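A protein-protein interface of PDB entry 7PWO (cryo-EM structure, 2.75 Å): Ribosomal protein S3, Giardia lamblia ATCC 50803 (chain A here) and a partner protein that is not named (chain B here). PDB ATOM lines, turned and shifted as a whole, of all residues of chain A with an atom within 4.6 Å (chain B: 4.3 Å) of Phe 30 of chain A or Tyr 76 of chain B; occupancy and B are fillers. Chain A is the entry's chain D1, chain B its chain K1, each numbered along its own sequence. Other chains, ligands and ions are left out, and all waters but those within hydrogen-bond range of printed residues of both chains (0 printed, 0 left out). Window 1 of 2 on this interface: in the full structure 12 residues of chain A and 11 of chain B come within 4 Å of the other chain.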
ATOM      1  N   GLU A  26       7.932  -8.663  29.854  1.00  0.00           N
ATOM      2  CA  GLU A  26       8.234  -9.673  28.842  1.00  0.00           C
ATOM      3  C   GLU A  26       9.655  -9.611  28.298  1.00  0.00           C
ATOM      4  O   GLU A  26      10.382 -10.611  28.308  1.00  0.00           O
ATOM      5  CB  GLU A  26       7.244  -9.553  27.685  1.00  0.00           C
ATOM      6  CG  GLU A  26       7.493 -10.581  26.593  1.00  0.00           C
ATOM      7  CD  GLU A  26       7.284 -12.000  27.041  1.00  0.00           C
ATOM      8  OE1 GLU A  26       6.509 -12.226  27.985  1.00  0.00           O
ATOM      9  OE2 GLU A  26       7.930 -12.890  26.453  1.00  0.00           O
ATOM     10  N   LEU A  27      10.040  -8.458  27.753  1.00  0.00           N
ATOM     11  CA  LEU A  27      11.333  -8.394  27.089  1.00  0.00           C
ATOM     12  C   LEU A  27      12.475  -8.587  28.078  1.00  0.00           C
ATOM     13  O   LEU A  27      13.443  -9.290  27.772  1.00  0.00           O
ATOM     14  CB  LEU A  27      11.482  -7.091  26.304  1.00  0.00           C
ATOM     15  CG  LEU A  27      10.278  -6.628  25.489  1.00  0.00           C
ATOM     16  CD1 LEU A  27      10.393  -5.146  25.159  1.00  0.00           C
ATOM     17  CD2 LEU A  27      10.134  -7.464  24.212  1.00  0.00           C
ATOM     18  N   HIS A  28      12.363  -8.021  29.285  1.00  0.00           N
ATOM     19  CA  HIS A  28      13.412  -8.257  30.273  1.00  0.00           C
ATOM     20  C   HIS A  28      13.530  -9.735  30.632  1.00  0.00           C
ATOM     21  O   HIS A  28      14.639 -10.274  30.694  1.00  0.00           O
ATOM     22  CB  HIS A  28      13.175  -7.437  31.537  1.00  0.00           C
ATOM     23  CG  HIS A  28      13.967  -7.918  32.717  1.00  0.00           C
ATOM     24  ND1 HIS A  28      15.192  -7.384  33.058  1.00  0.00           N
ATOM     25  CD2 HIS A  28      13.699  -8.863  33.648  1.00  0.00           C
ATOM     26  CE1 HIS A  28      15.649  -7.988  34.140  1.00  0.00           C
ATOM     27  NE2 HIS A  28      14.762  -8.890  34.518  1.00  0.00           N
ATOM     28  N   GLU A  29      12.411 -10.409  30.887  1.00  0.00           N
ATOM     29  CA  GLU A  29      12.521 -11.795  31.342  1.00  0.00           C
ATOM     30  C   GLU A  29      12.986 -12.714  30.216  1.00  0.00           C
ATOM     31  O   GLU A  29      13.757 -13.654  30.450  1.00  0.00           O
ATOM     32  CB  GLU A  29      11.199 -12.261  31.943  1.00  0.00           C
ATOM     33  CG  GLU A  29      10.068 -12.239  30.993  1.00  0.00           C
ATOM     34  CD  GLU A  29       9.973 -13.501  30.172  1.00  0.00           C
ATOM     35  OE1 GLU A  29      10.545 -14.539  30.589  1.00  0.00           O
ATOM     36  OE2 GLU A  29       9.305 -13.445  29.119  1.00  0.00           O
ATOM     37  N   PHE A  30      12.541 -12.454  28.984  1.00  0.00           N
ATOM     38  CA  PHE A  30      13.054 -13.211  27.850  1.00  0.00           C
ATOM     39  C   PHE A  30      14.553 -12.999  27.698  1.00  0.00           C
ATOM     40  O   PHE A  30      15.304 -13.949  27.448  1.00  0.00           O
ATOM     41  CB  PHE A  30      12.319 -12.809  26.571  1.00  0.00           C
ATOM     42  CG  PHE A  30      12.990 -13.293  25.312  1.00  0.00           C
ATOM     43  CD1 PHE A  30      12.822 -14.604  24.875  1.00  0.00           C
ATOM     44  CD2 PHE A  30      13.805 -12.445  24.576  1.00  0.00           C
ATOM     45  CE1 PHE A  30      13.442 -15.047  23.719  1.00  0.00           C
ATOM     46  CE2 PHE A  30      14.431 -12.891  23.423  1.00  0.00           C
ATOM     47  CZ  PHE A  30      14.252 -14.186  22.995  1.00  0.00           C
ATOM     48  N   PHE A  31      15.008 -11.749  27.836  1.00  0.00           N
ATOM     49  CA  PHE A  31      16.433 -11.474  27.728  1.00  0.00           C
ATOM     50  C   PHE A  31      17.207 -12.138  28.859  1.00  0.00           C
ATOM     51  O   PHE A  31      18.376 -12.489  28.684  1.00  0.00           O
ATOM     52  CB  PHE A  31      16.673  -9.962  27.723  1.00  0.00           C
ATOM     53  CG  PHE A  31      16.435  -9.310  26.396  1.00  0.00           C
ATOM     54  CD1 PHE A  31      16.353 -10.064  25.240  1.00  0.00           C
ATOM     55  CD2 PHE A  31      16.283  -7.933  26.302  1.00  0.00           C
ATOM     56  CE1 PHE A  31      16.133  -9.460  24.012  1.00  0.00           C
ATOM     57  CE2 PHE A  31      16.058  -7.328  25.077  1.00  0.00           C
ATOM     58  CZ  PHE A  31      15.983  -8.097  23.935  1.00  0.00           C
ATOM     59  N   SER A  32      16.575 -12.320  30.021  1.00  0.00           N
ATOM     60  CA  SER A  32      17.217 -13.019  31.128  1.00  0.00           C
ATOM     61  C   SER A  32      17.249 -14.523  30.904  1.00  0.00           C
ATOM     62  O   SER A  32      18.079 -15.219  31.496  1.00  0.00           O
ATOM     63  CB  SER A  32      16.508 -12.705  32.443  1.00  0.00           C
ATOM     64  OG  SER A  32      15.194 -13.225  32.450  1.00  0.00           O
ATOM     65  N   ARG A  33      16.318 -15.046  30.112  1.00  0.00           N
ATOM     66  CA  ARG A  33      16.407 -16.441  29.699  1.00  0.00           C
ATOM     67  C   ARG A  33      17.462 -16.643  28.612  1.00  0.00           C
ATOM     68  O   ARG A  33      18.119 -17.689  28.574  1.00  0.00           O
ATOM     69  CB  ARG A  33      15.035 -16.934  29.233  1.00  0.00           C
ATOM     70  CG  ARG A  33      13.987 -16.903  30.336  1.00  0.00           C
ATOM     71  CD  ARG A  33      14.454 -17.699  31.539  1.00  0.00           C
ATOM     72  NE  ARG A  33      13.850 -17.237  32.782  1.00  0.00           N
ATOM     73  CZ  ARG A  33      14.560 -16.771  33.807  1.00  0.00           C
ATOM     74  NH1 ARG A  33      15.880 -16.742  33.730  1.00  0.00           N
ATOM     75  NH2 ARG A  33      13.959 -16.357  34.913  1.00  0.00           N
ATOM     76  N   GLU A  34      17.641 -15.666  27.716  1.00  0.00           N
ATOM     77  CA  GLU A  34      18.399 -15.901  26.486  1.00  0.00           C
ATOM     78  C   GLU A  34      19.775 -15.243  26.473  1.00  0.00           C
ATOM     79  O   GLU A  34      20.775 -15.930  26.252  1.00  0.00           O
ATOM     80  CB  GLU A  34      17.589 -15.439  25.268  1.00  0.00           C
ATOM     81  CG  GLU A  34      18.003 -16.107  23.951  1.00  0.00           C
ATOM     82  CD  GLU A  34      19.395 -15.718  23.464  1.00  0.00           C
ATOM     83  OE1 GLU A  34      20.171 -16.614  23.073  1.00  0.00           O
ATOM     84  OE2 GLU A  34      19.706 -14.516  23.454  1.00  0.00           O
ATOM     85  N   LEU A  78      12.277 -10.934  15.791  1.00  0.00           N
ATOM     86  CA  LEU A  78      11.595 -11.774  16.761  1.00  0.00           C
ATOM     87  C   LEU A  78      10.873 -10.931  17.816  1.00  0.00           C
ATOM     88  O   LEU A  78      10.205 -11.479  18.697  1.00  0.00           O
ATOM     89  CB  LEU A  78      12.597 -12.736  17.410  1.00  0.00           C
ATOM     90  CG  LEU A  78      12.173 -13.807  18.421  1.00  0.00           C
ATOM     91  CD1 LEU A  78      11.237 -14.777  17.744  1.00  0.00           C
ATOM     92  CD2 LEU A  78      13.395 -14.537  18.948  1.00  0.00           C
ATOM     93  N   LEU B  22      10.622 -17.071  14.279  1.00  0.00           N
ATOM     94  CA  LEU B  22       9.336 -17.694  14.564  1.00  0.00           C
ATOM     95  C   LEU B  22       9.073 -17.792  16.067  1.00  0.00           C
ATOM     96  O   LEU B  22       9.991 -18.003  16.873  1.00  0.00           O
ATOM     97  CB  LEU B  22       9.267 -19.088  13.923  1.00  0.00           C
ATOM     98  CG  LEU B  22       7.972 -19.903  13.902  1.00  0.00           C
ATOM     99  CD1 LEU B  22       8.011 -20.835  12.712  1.00  0.00           C
ATOM    100  CD2 LEU B  22       7.712 -20.695  15.180  1.00  0.00           C
ATOM    101  N   LYS B  67      16.777 -23.754  16.833  1.00  0.00           N
ATOM    102  CA  LYS B  67      16.967 -23.860  18.276  1.00  0.00           C
ATOM    103  C   LYS B  67      15.887 -23.051  18.988  1.00  0.00           C
ATOM    104  O   LYS B  67      15.200 -22.237  18.369  1.00  0.00           O
ATOM    105  CB  LYS B  67      18.369 -23.371  18.652  1.00  0.00           C
ATOM    106  CG  LYS B  67      18.580 -21.893  18.376  1.00  0.00           C
ATOM    107  CD  LYS B  67      19.992 -21.463  18.708  1.00  0.00           C
ATOM    108  CE  LYS B  67      20.187 -19.975  18.442  1.00  0.00           C
ATOM    109  NZ  LYS B  67      21.575 -19.530  18.753  1.00  0.00           N
ATOM    110  N   ASP B  68      15.719 -23.261  20.299  1.00  0.00           N
ATOM    111  CA  ASP B  68      14.665 -22.541  21.008  1.00  0.00           C
ATOM    112  C   ASP B  68      15.094 -22.107  22.406  1.00  0.00           C
ATOM    113  O   ASP B  68      15.965 -22.708  23.044  1.00  0.00           O
ATOM    114  CB  ASP B  68      13.364 -23.363  21.124  1.00  0.00           C
ATOM    115  CG  ASP B  68      13.525 -24.643  21.939  1.00  0.00           C
ATOM    116  OD1 ASP B  68      14.638 -24.958  22.403  1.00  0.00           O
ATOM    117  OD2 ASP B  68      12.516 -25.346  22.120  1.00  0.00           O
ATOM    118  N   THR B  69      14.471 -21.016  22.849  1.00  0.00           N
ATOM    119  CA  THR B  69      14.346 -20.663  24.259  1.00  0.00           C
ATOM    120  C   THR B  69      12.858 -20.585  24.571  1.00  0.00           C
ATOM    121  O   THR B  69      12.031 -20.981  23.744  1.00  0.00           O
ATOM    122  CB  THR B  69      15.050 -19.342  24.588  1.00  0.00           C
ATOM    123  OG1 THR B  69      14.454 -18.280  23.837  1.00  0.00           O
ATOM    124  CG2 THR B  69      16.539 -19.424  24.267  1.00  0.00           C
ATOM    125  N   PHE B  70      12.493 -20.092  25.747  1.00  0.00           N
ATOM    126  CA  PHE B  70      11.094 -20.144  26.149  1.00  0.00           C
ATOM    127  C   PHE B  70      10.862 -19.075  27.211  1.00  0.00           C
ATOM    128  O   PHE B  70      11.710 -18.873  28.081  1.00  0.00           O
ATOM    129  CB  PHE B  70      10.762 -21.562  26.652  1.00  0.00           C
ATOM    130  CG  PHE B  70       9.327 -21.772  27.061  1.00  0.00           C
ATOM    131  CD1 PHE B  70       8.331 -21.909  26.103  1.00  0.00           C
ATOM    132  CD2 PHE B  70       8.991 -21.936  28.391  1.00  0.00           C
ATOM    133  CE1 PHE B  70       7.015 -22.130  26.472  1.00  0.00           C
ATOM    134  CE2 PHE B  70       7.681 -22.164  28.771  1.00  0.00           C
ATOM    135  CZ  PHE B  70       6.690 -22.268  27.812  1.00  0.00           C
ATOM    136  N   ALA B  71       9.730 -18.379  27.119  1.00  0.00           N
ATOM    137  CA  ALA B  71       9.424 -17.300  28.056  1.00  0.00           C
ATOM    138  C   ALA B  71       7.928 -17.029  28.039  1.00  0.00           C
ATOM    139  O   ALA B  71       7.394 -16.613  27.008  1.00  0.00           O
ATOM    140  CB  ALA B  71      10.211 -16.033  27.699  1.00  0.00           C
ATOM    141  N   HIS B  74       5.438 -19.170  25.602  1.00  0.00           N
ATOM    142  CA  HIS B  74       5.636 -18.708  24.234  1.00  0.00           C
ATOM    143  C   HIS B  74       6.957 -19.278  23.737  1.00  0.00           C
ATOM    144  O   HIS B  74       8.025 -18.844  24.170  1.00  0.00           O
ATOM    145  CB  HIS B  74       5.632 -17.189  24.183  1.00  0.00           C
ATOM    146  CG  HIS B  74       5.095 -16.624  22.907  1.00  0.00           C
ATOM    147  ND1 HIS B  74       4.818 -15.285  22.753  1.00  0.00           N
ATOM    148  CD2 HIS B  74       4.784 -17.212  21.728  1.00  0.00           C
ATOM    149  CE1 HIS B  74       4.357 -15.072  21.534  1.00  0.00           C
ATOM    150  NE2 HIS B  74       4.326 -16.225  20.892  1.00  0.00           N
ATOM    151  N   HIS B  75       6.882 -20.275  22.866  1.00  0.00           N
ATOM    152  CA  HIS B  75       8.071 -20.809  22.230  1.00  0.00           C
ATOM    153  C   HIS B  75       8.726 -19.738  21.369  1.00  0.00           C
ATOM    154  O   HIS B  75       8.060 -19.092  20.559  1.00  0.00           O
ATOM    155  CB  HIS B  75       7.699 -22.013  21.368  1.00  0.00           C
ATOM    156  CG  HIS B  75       7.555 -23.290  22.132  1.00  0.00           C
ATOM    157  ND1 HIS B  75       8.212 -23.527  23.318  1.00  0.00           N
ATOM    158  CD2 HIS B  75       6.855 -24.416  21.859  1.00  0.00           C
ATOM    159  CE1 HIS B  75       7.909 -24.736  23.753  1.00  0.00           C
ATOM    160  NE2 HIS B  75       7.092 -25.300  22.882  1.00  0.00           N
ATOM    161  N   TYR B  76      10.027 -19.548  21.552  1.00  0.00           N
ATOM    162  CA  TYR B  76      10.829 -18.669  20.708  1.00  0.00           C
ATOM    163  C   TYR B  76      11.889 -19.500  20.008  1.00  0.00           C
ATOM    164  O   TYR B  76      12.636 -20.237  20.666  1.00  0.00           O
ATOM    165  CB  TYR B  76      11.499 -17.548  21.513  1.00  0.00           C
ATOM    166  CG  TYR B  76      10.544 -16.642  22.241  1.00  0.00           C
ATOM    167  CD1 TYR B  76      10.127 -16.932  23.536  1.00  0.00           C
ATOM    168  CD2 TYR B  76      10.043 -15.497  21.626  1.00  0.00           C
ATOM    169  CE1 TYR B  76       9.232 -16.100  24.203  1.00  0.00           C
ATOM    170  CE2 TYR B  76       9.164 -14.658  22.281  1.00  0.00           C
ATOM    171  CZ  TYR B  76       8.749 -14.968  23.566  1.00  0.00           C
ATOM    172  OH  TYR B  76       7.868 -14.137  24.212  1.00  0.00           O
ATOM    173  N   TYR B  77      11.978 -19.359  18.686  1.00  0.00           N
ATOM    174  CA  TYR B  77      12.940 -20.109  17.899  1.00  0.00           C
ATOM    175  C   TYR B  77      14.000 -19.170  17.343  1.00  0.00           C
ATOM    176  O   TYR B  77      13.844 -17.945  17.350  1.00  0.00           O
ATOM    177  CB  TYR B  77      12.227 -20.847  16.769  1.00  0.00           C
ATOM    178  CG  TYR B  77      11.287 -21.907  17.291  1.00  0.00           C
ATOM    179  CD1 TYR B  77      11.739 -23.185  17.584  1.00  0.00           C
ATOM    180  CD2 TYR B  77       9.958 -21.612  17.534  1.00  0.00           C
ATOM    181  CE1 TYR B  77      10.880 -24.146  18.075  1.00  0.00           C
ATOM    182  CE2 TYR B  77       9.096 -22.563  18.025  1.00  0.00           C
ATOM    183  CZ  TYR B  77       9.559 -23.828  18.296  1.00  0.00           C
ATOM    184  OH  TYR B  77       8.699 -24.778  18.787  1.00  0.00           O
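The backbone NH of Thr 69 of chain B is in hydrogen-bond range of the backbone carbonyl oxygen of Tyr 76 of chain B (3.0 Å).
The backbone carbonyl oxygen (O) of Glu 29 of chain A sits at hydrogen-bond distance from the side-chain hydroxyl (OG) of Ser 32 of chain A.
N of Tyr 77 of chain B sits at hydrogen-bond distance from O of Leu 22 of chain B (3.0 Å).
Of the printed residues of chain B, Glu 29 of chain A touches Ala 71 (3.1 Å).
Printed residues of chain B within 4 Å of Phe 30 of chain A: Thr 69 and Tyr 76.
Of the printed residues of chain B, Leu 78 of chain A touches Leu 22 (3.6 Å) and Tyr 77 (3.8 Å).
Printed residues of chain A within 4 Å of Tyr 76 of chain B: Glu 26 (2.6 Å) and Phe 30 (3.6 Å).
Glu 26 of chain A touches Ala 71 of chain B (OE2 to O, 3.8 Å).
Glu 29 of chain A touches Ala 71 of chain B.
CE1 of Phe 30 of chain A touches OG1 of Thr 69 of chain B, 3.4 Å away.
CG of Tyr 76 of chain B touches CE1 of Phe 30 of chain A, 3.6 Å away.
CG of Arg 33 of chain A touches O of Phe 70 of chain B (3.8 Å).
Glu 34 of chain A touches Thr 69 of chain B.
O of Leu 22 of chain B touches CD1 of Leu 78 of chain A (3.6 Å).
Tyr 77 of chain B touches Leu 78 of chain A (O to CD2, 3.8 Å).
OH of Tyr 76 of chain B sits at hydrogen-bond distance from OE2 of Glu 26 of chain A (2.6 Å).
Of the 10 printed residues of chain B, 6 touch a printed residue of chain A.
Hydrophobic or aromatic side chains of chain B that line the printed part of chain A: Ala 71 and Tyr 76.
Printed residues of chain A that touch a printed residue of chain B: Glu 26, Glu 29, Phe 30, Arg 33, Glu 34 and Leu 78.
Along chain A the printed residues that touch a printed residue of chain B span positions 26 to 78.
Among the printed residues, 9 pairs touch across the chains.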
